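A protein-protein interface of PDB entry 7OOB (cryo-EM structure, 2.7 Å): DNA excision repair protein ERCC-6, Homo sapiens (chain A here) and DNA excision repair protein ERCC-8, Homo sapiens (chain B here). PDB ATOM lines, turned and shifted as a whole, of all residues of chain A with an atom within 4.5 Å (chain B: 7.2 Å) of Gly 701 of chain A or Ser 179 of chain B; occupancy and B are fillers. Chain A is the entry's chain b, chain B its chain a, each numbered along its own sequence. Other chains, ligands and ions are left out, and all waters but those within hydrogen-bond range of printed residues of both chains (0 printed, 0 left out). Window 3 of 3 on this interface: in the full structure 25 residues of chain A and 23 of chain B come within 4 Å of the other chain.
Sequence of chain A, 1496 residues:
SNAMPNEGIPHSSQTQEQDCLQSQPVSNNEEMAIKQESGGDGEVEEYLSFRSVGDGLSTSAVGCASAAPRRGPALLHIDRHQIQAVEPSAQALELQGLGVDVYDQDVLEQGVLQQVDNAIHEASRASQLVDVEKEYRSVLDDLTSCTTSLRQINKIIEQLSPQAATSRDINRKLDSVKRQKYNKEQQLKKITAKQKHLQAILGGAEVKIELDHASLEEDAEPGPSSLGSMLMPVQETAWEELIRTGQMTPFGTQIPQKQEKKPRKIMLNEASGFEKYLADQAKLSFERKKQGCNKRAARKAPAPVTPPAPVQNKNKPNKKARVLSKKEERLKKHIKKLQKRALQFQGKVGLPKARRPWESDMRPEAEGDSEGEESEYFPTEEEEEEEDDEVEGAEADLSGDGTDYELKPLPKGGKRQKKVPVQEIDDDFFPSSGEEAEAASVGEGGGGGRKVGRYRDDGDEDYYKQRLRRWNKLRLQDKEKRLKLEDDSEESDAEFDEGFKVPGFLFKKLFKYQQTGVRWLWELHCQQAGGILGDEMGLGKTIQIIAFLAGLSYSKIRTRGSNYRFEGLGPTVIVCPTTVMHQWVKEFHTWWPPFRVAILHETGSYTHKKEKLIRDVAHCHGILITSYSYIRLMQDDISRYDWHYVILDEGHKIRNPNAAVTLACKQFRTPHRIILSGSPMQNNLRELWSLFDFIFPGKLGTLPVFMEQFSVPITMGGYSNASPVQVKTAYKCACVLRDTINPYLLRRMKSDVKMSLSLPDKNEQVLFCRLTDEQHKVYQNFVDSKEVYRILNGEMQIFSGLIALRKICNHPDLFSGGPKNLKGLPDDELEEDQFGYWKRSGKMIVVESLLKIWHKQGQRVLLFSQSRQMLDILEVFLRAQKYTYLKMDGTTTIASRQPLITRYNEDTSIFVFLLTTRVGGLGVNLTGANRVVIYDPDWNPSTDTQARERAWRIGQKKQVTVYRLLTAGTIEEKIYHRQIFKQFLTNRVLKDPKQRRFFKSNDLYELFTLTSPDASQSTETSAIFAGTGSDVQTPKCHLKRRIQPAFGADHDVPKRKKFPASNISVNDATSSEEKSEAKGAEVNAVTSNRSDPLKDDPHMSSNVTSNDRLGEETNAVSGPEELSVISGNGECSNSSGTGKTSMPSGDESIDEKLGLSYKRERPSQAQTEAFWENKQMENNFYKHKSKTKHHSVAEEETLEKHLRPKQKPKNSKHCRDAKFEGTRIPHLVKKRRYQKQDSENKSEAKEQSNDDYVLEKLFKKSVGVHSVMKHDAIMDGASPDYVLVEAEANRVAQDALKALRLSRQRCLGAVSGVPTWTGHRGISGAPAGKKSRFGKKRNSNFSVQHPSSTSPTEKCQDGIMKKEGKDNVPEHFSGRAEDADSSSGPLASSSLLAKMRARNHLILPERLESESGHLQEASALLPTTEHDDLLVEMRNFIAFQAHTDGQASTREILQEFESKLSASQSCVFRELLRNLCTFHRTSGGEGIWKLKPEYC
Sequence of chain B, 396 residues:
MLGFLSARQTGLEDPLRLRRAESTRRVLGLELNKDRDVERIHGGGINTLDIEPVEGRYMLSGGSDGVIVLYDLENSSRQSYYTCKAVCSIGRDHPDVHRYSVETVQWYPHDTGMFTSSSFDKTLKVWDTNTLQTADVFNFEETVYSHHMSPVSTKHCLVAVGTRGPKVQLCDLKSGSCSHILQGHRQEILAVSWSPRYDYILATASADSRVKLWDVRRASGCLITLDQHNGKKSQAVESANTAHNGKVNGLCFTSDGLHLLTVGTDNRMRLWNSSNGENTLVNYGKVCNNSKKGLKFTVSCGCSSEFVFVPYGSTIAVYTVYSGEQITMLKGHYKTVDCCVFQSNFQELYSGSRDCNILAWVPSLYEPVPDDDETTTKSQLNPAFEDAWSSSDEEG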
ATOM      1  N   TRP A 689      17.858  20.137  15.824  1.00  0.00           N
ATOM      2  CA  TRP A 689      18.168  21.110  16.860  1.00  0.00           C
ATOM      3  C   TRP A 689      16.901  21.628  17.510  1.00  0.00           C
ATOM      4  O   TRP A 689      16.863  21.826  18.722  1.00  0.00           O
ATOM      5  CB  TRP A 689      18.966  22.287  16.314  1.00  0.00           C
ATOM      6  CG  TRP A 689      19.302  23.262  17.416  1.00  0.00           C
ATOM      7  CD1 TRP A 689      20.410  23.253  18.206  1.00  0.00           C
ATOM      8  CD2 TRP A 689      18.498  24.356  17.871  1.00  0.00           C
ATOM      9  NE1 TRP A 689      20.355  24.281  19.114  1.00  0.00           N
ATOM     10  CE2 TRP A 689      19.189  24.974  18.927  1.00  0.00           C
ATOM     11  CE3 TRP A 689      17.262  24.878  17.479  1.00  0.00           C
ATOM     12  CZ2 TRP A 689      18.689  26.084  19.595  1.00  0.00           C
ATOM     13  CZ3 TRP A 689      16.770  25.979  18.143  1.00  0.00           C
ATOM     14  CH2 TRP A 689      17.481  26.570  19.189  1.00  0.00           C
ATOM     15  N   PRO A 697      17.011  22.184  26.345  1.00  0.00           N
ATOM     16  CA  PRO A 697      17.447  23.385  25.615  1.00  0.00           C
ATOM     17  C   PRO A 697      18.941  23.527  25.396  1.00  0.00           C
ATOM     18  O   PRO A 697      19.348  24.051  24.353  1.00  0.00           O
ATOM     19  CB  PRO A 697      16.904  24.509  26.503  1.00  0.00           C
ATOM     20  CG  PRO A 697      15.664  23.958  27.031  1.00  0.00           C
ATOM     21  CD  PRO A 697      15.914  22.511  27.259  1.00  0.00           C
ATOM     22  N   GLY A 698      19.771  23.101  26.341  1.00  0.00           N
ATOM     23  CA  GLY A 698      21.180  23.406  26.234  1.00  0.00           C
ATOM     24  C   GLY A 698      22.063  22.429  25.487  1.00  0.00           C
ATOM     25  O   GLY A 698      23.104  22.870  25.000  1.00  0.00           O
ATOM     26  N   LYS A 699      21.664  21.159  25.306  1.00  0.00           N
ATOM     27  CA  LYS A 699      22.615  20.110  24.920  1.00  0.00           C
ATOM     28  C   LYS A 699      23.291  20.476  23.619  1.00  0.00           C
ATOM     29  O   LYS A 699      24.491  20.755  23.576  1.00  0.00           O
ATOM     30  CB  LYS A 699      21.942  18.740  24.725  1.00  0.00           C
ATOM     31  CG  LYS A 699      22.846  17.598  24.346  1.00  0.00           C
ATOM     32  CD  LYS A 699      23.894  17.314  25.427  1.00  0.00           C
ATOM     33  CE  LYS A 699      23.276  16.831  26.737  1.00  0.00           C
ATOM     34  NZ  LYS A 699      24.134  15.854  27.441  1.00  0.00           N
ATOM     35  N   LEU A 700      22.508  20.480  22.558  1.00  0.00           N
ATOM     36  CA  LEU A 700      22.894  21.215  21.381  1.00  0.00           C
ATOM     37  C   LEU A 700      22.816  22.682  21.763  1.00  0.00           C
ATOM     38  O   LEU A 700      21.918  23.096  22.501  1.00  0.00           O
ATOM     39  CB  LEU A 700      21.969  20.860  20.218  1.00  0.00           C
ATOM     40  CG  LEU A 700      21.595  19.367  20.132  1.00  0.00           C
ATOM     41  CD1 LEU A 700      20.760  19.093  18.923  1.00  0.00           C
ATOM     42  CD2 LEU A 700      22.821  18.450  20.150  1.00  0.00           C
ATOM     43  N   GLY A 701      23.780  23.465  21.307  1.00  0.00           N
ATOM     44  CA  GLY A 701      23.961  24.767  21.911  1.00  0.00           C
ATOM     45  C   GLY A 701      22.878  25.735  21.499  1.00  0.00           C
ATOM     46  O   GLY A 701      21.712  25.360  21.352  1.00  0.00           O
ATOM     47  N   THR A 702      23.237  26.999  21.345  1.00  0.00           N
ATOM     48  CA  THR A 702      22.388  27.881  20.572  1.00  0.00           C
ATOM     49  C   THR A 702      22.482  27.475  19.109  1.00  0.00           C
ATOM     50  O   THR A 702      23.462  26.864  18.674  1.00  0.00           O
ATOM     51  CB  THR A 702      22.800  29.336  20.757  1.00  0.00           C
ATOM     52  OG1 THR A 702      24.148  29.512  20.309  1.00  0.00           O
ATOM     53  CG2 THR A 702      22.688  29.738  22.217  1.00  0.00           C
ATOM     54  N   LEU A 703      21.439  27.784  18.356  1.00  0.00           N
ATOM     55  CA  LEU A 703      21.412  27.461  16.938  1.00  0.00           C
ATOM     56  C   LEU A 703      22.633  27.988  16.186  1.00  0.00           C
ATOM     57  O   LEU A 703      23.079  27.339  15.233  1.00  0.00           O
ATOM     58  CB  LEU A 703      20.124  27.997  16.310  1.00  0.00           C
ATOM     59  CG  LEU A 703      19.654  27.434  14.962  1.00  0.00           C
ATOM     60  CD1 LEU A 703      19.809  25.926  14.823  1.00  0.00           C
ATOM     61  CD2 LEU A 703      18.201  27.822  14.759  1.00  0.00           C
ATOM     62  N   PHE A 710      27.908  21.561  13.486  1.00  0.00           N
ATOM     63  CA  PHE A 710      27.347  20.305  13.005  1.00  0.00           C
ATOM     64  C   PHE A 710      26.710  20.423  11.633  1.00  0.00           C
ATOM     65  O   PHE A 710      26.985  19.597  10.757  1.00  0.00           O
ATOM     66  CB  PHE A 710      26.302  19.795  14.007  1.00  0.00           C
ATOM     67  CG  PHE A 710      26.878  19.391  15.322  1.00  0.00           C
ATOM     68  CD1 PHE A 710      27.531  18.186  15.460  1.00  0.00           C
ATOM     69  CD2 PHE A 710      26.753  20.213  16.426  1.00  0.00           C
ATOM     70  CE1 PHE A 710      28.059  17.810  16.672  1.00  0.00           C
ATOM     71  CE2 PHE A 710      27.280  19.840  17.638  1.00  0.00           C
ATOM     72  CZ  PHE A 710      27.933  18.638  17.761  1.00  0.00           C
ATOM     73  N   THR A 740      26.329  12.786  21.405  1.00  0.00           N
ATOM     74  CA  THR A 740      25.712  13.814  22.229  1.00  0.00           C
ATOM     75  C   THR A 740      24.235  13.520  22.446  1.00  0.00           C
ATOM     76  O   THR A 740      23.724  13.671  23.562  1.00  0.00           O
ATOM     77  CB  THR A 740      25.899  15.183  21.577  1.00  0.00           C
ATOM     78  OG1 THR A 740      27.283  15.381  21.265  1.00  0.00           O
ATOM     79  CG2 THR A 740      25.450  16.283  22.508  1.00  0.00           C
ATOM     80  N   VAL B 168      27.825  29.124  30.517  1.00  0.00           N
ATOM     81  CA  VAL B 168      28.822  28.177  31.001  1.00  0.00           C
ATOM     82  C   VAL B 168      28.900  27.043  29.994  1.00  0.00           C
ATOM     83  O   VAL B 168      27.906  26.351  29.754  1.00  0.00           O
ATOM     84  CB  VAL B 168      28.465  27.647  32.399  1.00  0.00           C
ATOM     85  CG1 VAL B 168      29.582  26.758  32.941  1.00  0.00           C
ATOM     86  CG2 VAL B 168      28.170  28.789  33.351  1.00  0.00           C
ATOM     87  N   GLN B 169      30.079  26.833  29.423  1.00  0.00           N
ATOM     88  CA  GLN B 169      30.274  25.794  28.423  1.00  0.00           C
ATOM     89  C   GLN B 169      30.601  24.480  29.115  1.00  0.00           C
ATOM     90  O   GLN B 169      31.458  24.437  29.995  1.00  0.00           O
ATOM     91  CB  GLN B 169      31.403  26.163  27.459  1.00  0.00           C
ATOM     92  CG  GLN B 169      31.387  27.597  26.924  1.00  0.00           C
ATOM     93  CD  GLN B 169      30.436  27.780  25.765  1.00  0.00           C
ATOM     94  OE1 GLN B 169      29.543  28.626  25.809  1.00  0.00           O
ATOM     95  NE2 GLN B 169      30.629  26.998  24.709  1.00  0.00           N
ATOM     96  N   LEU B 170      29.915  23.413  28.732  1.00  0.00           N
ATOM     97  CA  LEU B 170      30.255  22.076  29.198  1.00  0.00           C
ATOM     98  C   LEU B 170      30.844  21.310  28.024  1.00  0.00           C
ATOM     99  O   LEU B 170      30.186  21.144  26.993  1.00  0.00           O
ATOM    100  CB  LEU B 170      29.034  21.363  29.774  1.00  0.00           C
ATOM    101  CG  LEU B 170      28.374  21.972  31.014  1.00  0.00           C
ATOM    102  CD1 LEU B 170      27.243  21.087  31.475  1.00  0.00           C
ATOM    103  CD2 LEU B 170      29.359  22.200  32.145  1.00  0.00           C
ATOM    104  N   CYS B 171      32.088  20.863  28.179  1.00  0.00           N
ATOM    105  CA  CYS B 171      32.811  20.142  27.139  1.00  0.00           C
ATOM    106  C   CYS B 171      32.968  18.694  27.570  1.00  0.00           C
ATOM    107  O   CYS B 171      33.585  18.419  28.600  1.00  0.00           O
ATOM    108  CB  CYS B 171      34.181  20.774  26.896  1.00  0.00           C
ATOM    109  SG  CYS B 171      34.131  22.538  26.538  1.00  0.00           S
ATOM    110  N   ASP B 172      32.443  17.772  26.773  1.00  0.00           N
ATOM    111  CA  ASP B 172      32.556  16.349  27.068  1.00  0.00           C
ATOM    112  C   ASP B 172      33.846  15.839  26.441  1.00  0.00           C
ATOM    113  O   ASP B 172      34.000  15.865  25.219  1.00  0.00           O
ATOM    114  CB  ASP B 172      31.341  15.591  26.535  1.00  0.00           C
ATOM    115  CG  ASP B 172      31.009  14.351  27.351  1.00  0.00           C
ATOM    116  OD1 ASP B 172      31.418  14.256  28.527  1.00  0.00           O
ATOM    117  OD2 ASP B 172      30.323  13.462  26.808  1.00  0.00           O
ATOM    118  N   GLY B 176      33.855  14.345  21.685  1.00  0.00           N
ATOM    119  CA  GLY B 176      34.022  15.759  21.961  1.00  0.00           C
ATOM    120  C   GLY B 176      32.794  16.595  21.686  1.00  0.00           C
ATOM    121  O   GLY B 176      32.505  16.914  20.532  1.00  0.00           O
ATOM    122  N   SER B 177      32.101  17.008  22.744  1.00  0.00           N
ATOM    123  CA  SER B 177      30.820  17.703  22.633  1.00  0.00           C
ATOM    124  C   SER B 177      30.907  18.991  23.444  1.00  0.00           C
ATOM    125  O   SER B 177      30.726  18.978  24.664  1.00  0.00           O
ATOM    126  CB  SER B 177      29.679  16.817  23.118  1.00  0.00           C
ATOM    127  OG  SER B 177      29.618  15.617  22.368  1.00  0.00           O
ATOM    128  N   CYS B 178      31.179  20.101  22.758  1.00  0.00           N
ATOM    129  CA  CYS B 178      31.225  21.424  23.366  1.00  0.00           C
ATOM    130  C   CYS B 178      29.988  22.247  23.033  1.00  0.00           C
ATOM    131  O   CYS B 178      30.078  23.470  22.881  1.00  0.00           O
ATOM    132  CB  CYS B 178      32.484  22.165  22.921  1.00  0.00           C
ATOM    133  SG  CYS B 178      32.579  22.458  21.141  1.00  0.00           S
ATOM    134  N   SER B 179      28.835  21.596  22.907  1.00  0.00           N
ATOM    135  CA  SER B 179      27.593  22.282  22.577  1.00  0.00           C
ATOM    136  C   SER B 179      26.789  22.641  23.819  1.00  0.00           C
ATOM    137  O   SER B 179      26.134  23.687  23.850  1.00  0.00           O
ATOM    138  CB  SER B 179      26.751  21.410  21.645  1.00  0.00           C
ATOM    139  OG  SER B 179      26.491  20.147  22.226  1.00  0.00           O
ATOM    140  N   HIS B 180      26.832  21.792  24.843  1.00  0.00           N
ATOM    141  CA  HIS B 180      26.038  22.012  26.043  1.00  0.00           C
ATOM    142  C   HIS B 180      26.433  23.323  26.713  1.00  0.00           C
ATOM    143  O   HIS B 180      27.617  23.586  26.943  1.00  0.00           O
ATOM    144  CB  HIS B 180      26.225  20.834  26.995  1.00  0.00           C
ATOM    145  CG  HIS B 180      25.233  20.778  28.117  1.00  0.00           C
ATOM    146  ND1 HIS B 180      25.112  19.679  28.938  1.00  0.00           N
ATOM    147  CD2 HIS B 180      24.309  21.670  28.546  1.00  0.00           C
ATOM    148  CE1 HIS B 180      24.167  19.902  29.833  1.00  0.00           C
ATOM    149  NE2 HIS B 180      23.663  21.103  29.616  1.00  0.00           N
ATOM    150  N   ILE B 181      25.433  24.143  27.030  1.00  0.00           N
ATOM    151  CA  ILE B 181      25.638  25.447  27.647  1.00  0.00           C
ATOM    152  C   ILE B 181      24.610  25.629  28.756  1.00  0.00           C
ATOM    153  O   ILE B 181      23.437  25.283  28.592  1.00  0.00           O
ATOM    154  CB  ILE B 181      25.535  26.589  26.616  1.00  0.00           C
ATOM    155  CG1 ILE B 181      24.263  26.438  25.772  1.00  0.00           C
ATOM    156  CG2 ILE B 181      26.773  26.599  25.731  1.00  0.00           C
ATOM    157  CD1 ILE B 181      23.912  27.653  24.959  1.00  0.00           C
ATOM    158  N   LEU B 182      25.057  26.162  29.891  1.00  0.00           N
ATOM    159  CA  LEU B 182      24.179  26.501  31.006  1.00  0.00           C
ATOM    160  C   LEU B 182      23.954  28.005  30.978  1.00  0.00           C
ATOM    161  O   LEU B 182      24.859  28.778  31.304  1.00  0.00           O
ATOM    162  CB  LEU B 182      24.788  26.079  32.340  1.00  0.00           C
ATOM    163  CG  LEU B 182      25.355  24.671  32.466  1.00  0.00           C
ATOM    164  CD1 LEU B 182      26.252  24.607  33.680  1.00  0.00           C
ATOM    165  CD2 LEU B 182      24.241  23.650  32.564  1.00  0.00           C
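The backbone NH of His 180 of chain B lies within hydrogen-bond range of the backbone carbonyl oxygen of Lys 699 of chain A (2.9 Å).
The backbone carbonyl oxygen of Lys 699 of chain A lies within hydrogen-bond range of the side-chain hydroxyl of Ser 179 of chain B (2.5 Å).
The side-chain hydroxyl of Ser 177 of chain B is in hydrogen-bond range of the side-chain hydroxyl of Thr 740 of chain A, 2.6 Å away.
The backbone NH (N) of Gly 701 of chain A lies close to the backbone carbonyl oxygen (O) of Ser 179 of chain B, 3.5 Å away.
The backbone carbonyl oxygen (O) of Ser 179 of chain B sits close to the backbone carbonyl oxygen (O) of Gly 698 of chain A, 3.3 Å away.
The backbone carbonyl oxygen (O) of Gly 698 of chain A lies within hydrogen-bond range of the backbone NH (N) of Ile 181 of chain B (3.3 Å).
The backbone NH of Leu 170 of chain B sits at hydrogen-bond distance from the backbone carbonyl oxygen of His 180 of chain B (2.9 Å).
The indole nitrogen (NE1) of Trp 689 of chain A is in hydrogen-bond range of the backbone carbonyl oxygen (O) of Gly 701 of chain A (2.8 Å).
O of Ser 177 of chain B is in hydrogen-bond range of N of Asp 172 of chain B (3.0 Å).
Among the printed residues, pairs that only touch across the chains: Gly 698 of chain A with His 180 of chain B (3.2 Å), Thr 702 of chain A with Ile 181 of chain B (3.7 Å) and Leu 700 of chain A with Ser 179 of chain B (3.8 Å).
Gly 701 of chain A touches one residue of chain B.
Printed residues of chain A within 4 Å of Ser 179 of chain B: Gly 698 (3.3 Å), Lys 699 (2.5 Å), Leu 700 (3.8 Å) and Gly 701 (3.1 Å).
Of the printed residues of chain B, Thr 702 of chain A touches Ile 181.
Of the printed residues of chain B, Gly 698 of chain A touches Ser 179, His 180 and Ile 181.
Gln 169 of chain B touches none of the printed residues of chain A.
Leu 182 of chain B touches none of the printed residues of chain A.
The nearest printed residue of chain B that does not touch Lys 699 of chain A is Ile 181 of chain B (4.9 Å).
Of the 12 printed residues of chain B, 4 touch a printed residue of chain A.
Hydrophobic or aromatic side chains of chain B within 4 Å of the printed part of chain A: His 180 and Ile 181.
Of the 10 printed residues of chain A, 6 touch a printed residue of chain B.
Among the printed residues, no Asp or Glu carboxylate lies within 4 Å of a Lys or Arg side-chain nitrogen of the other chain.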
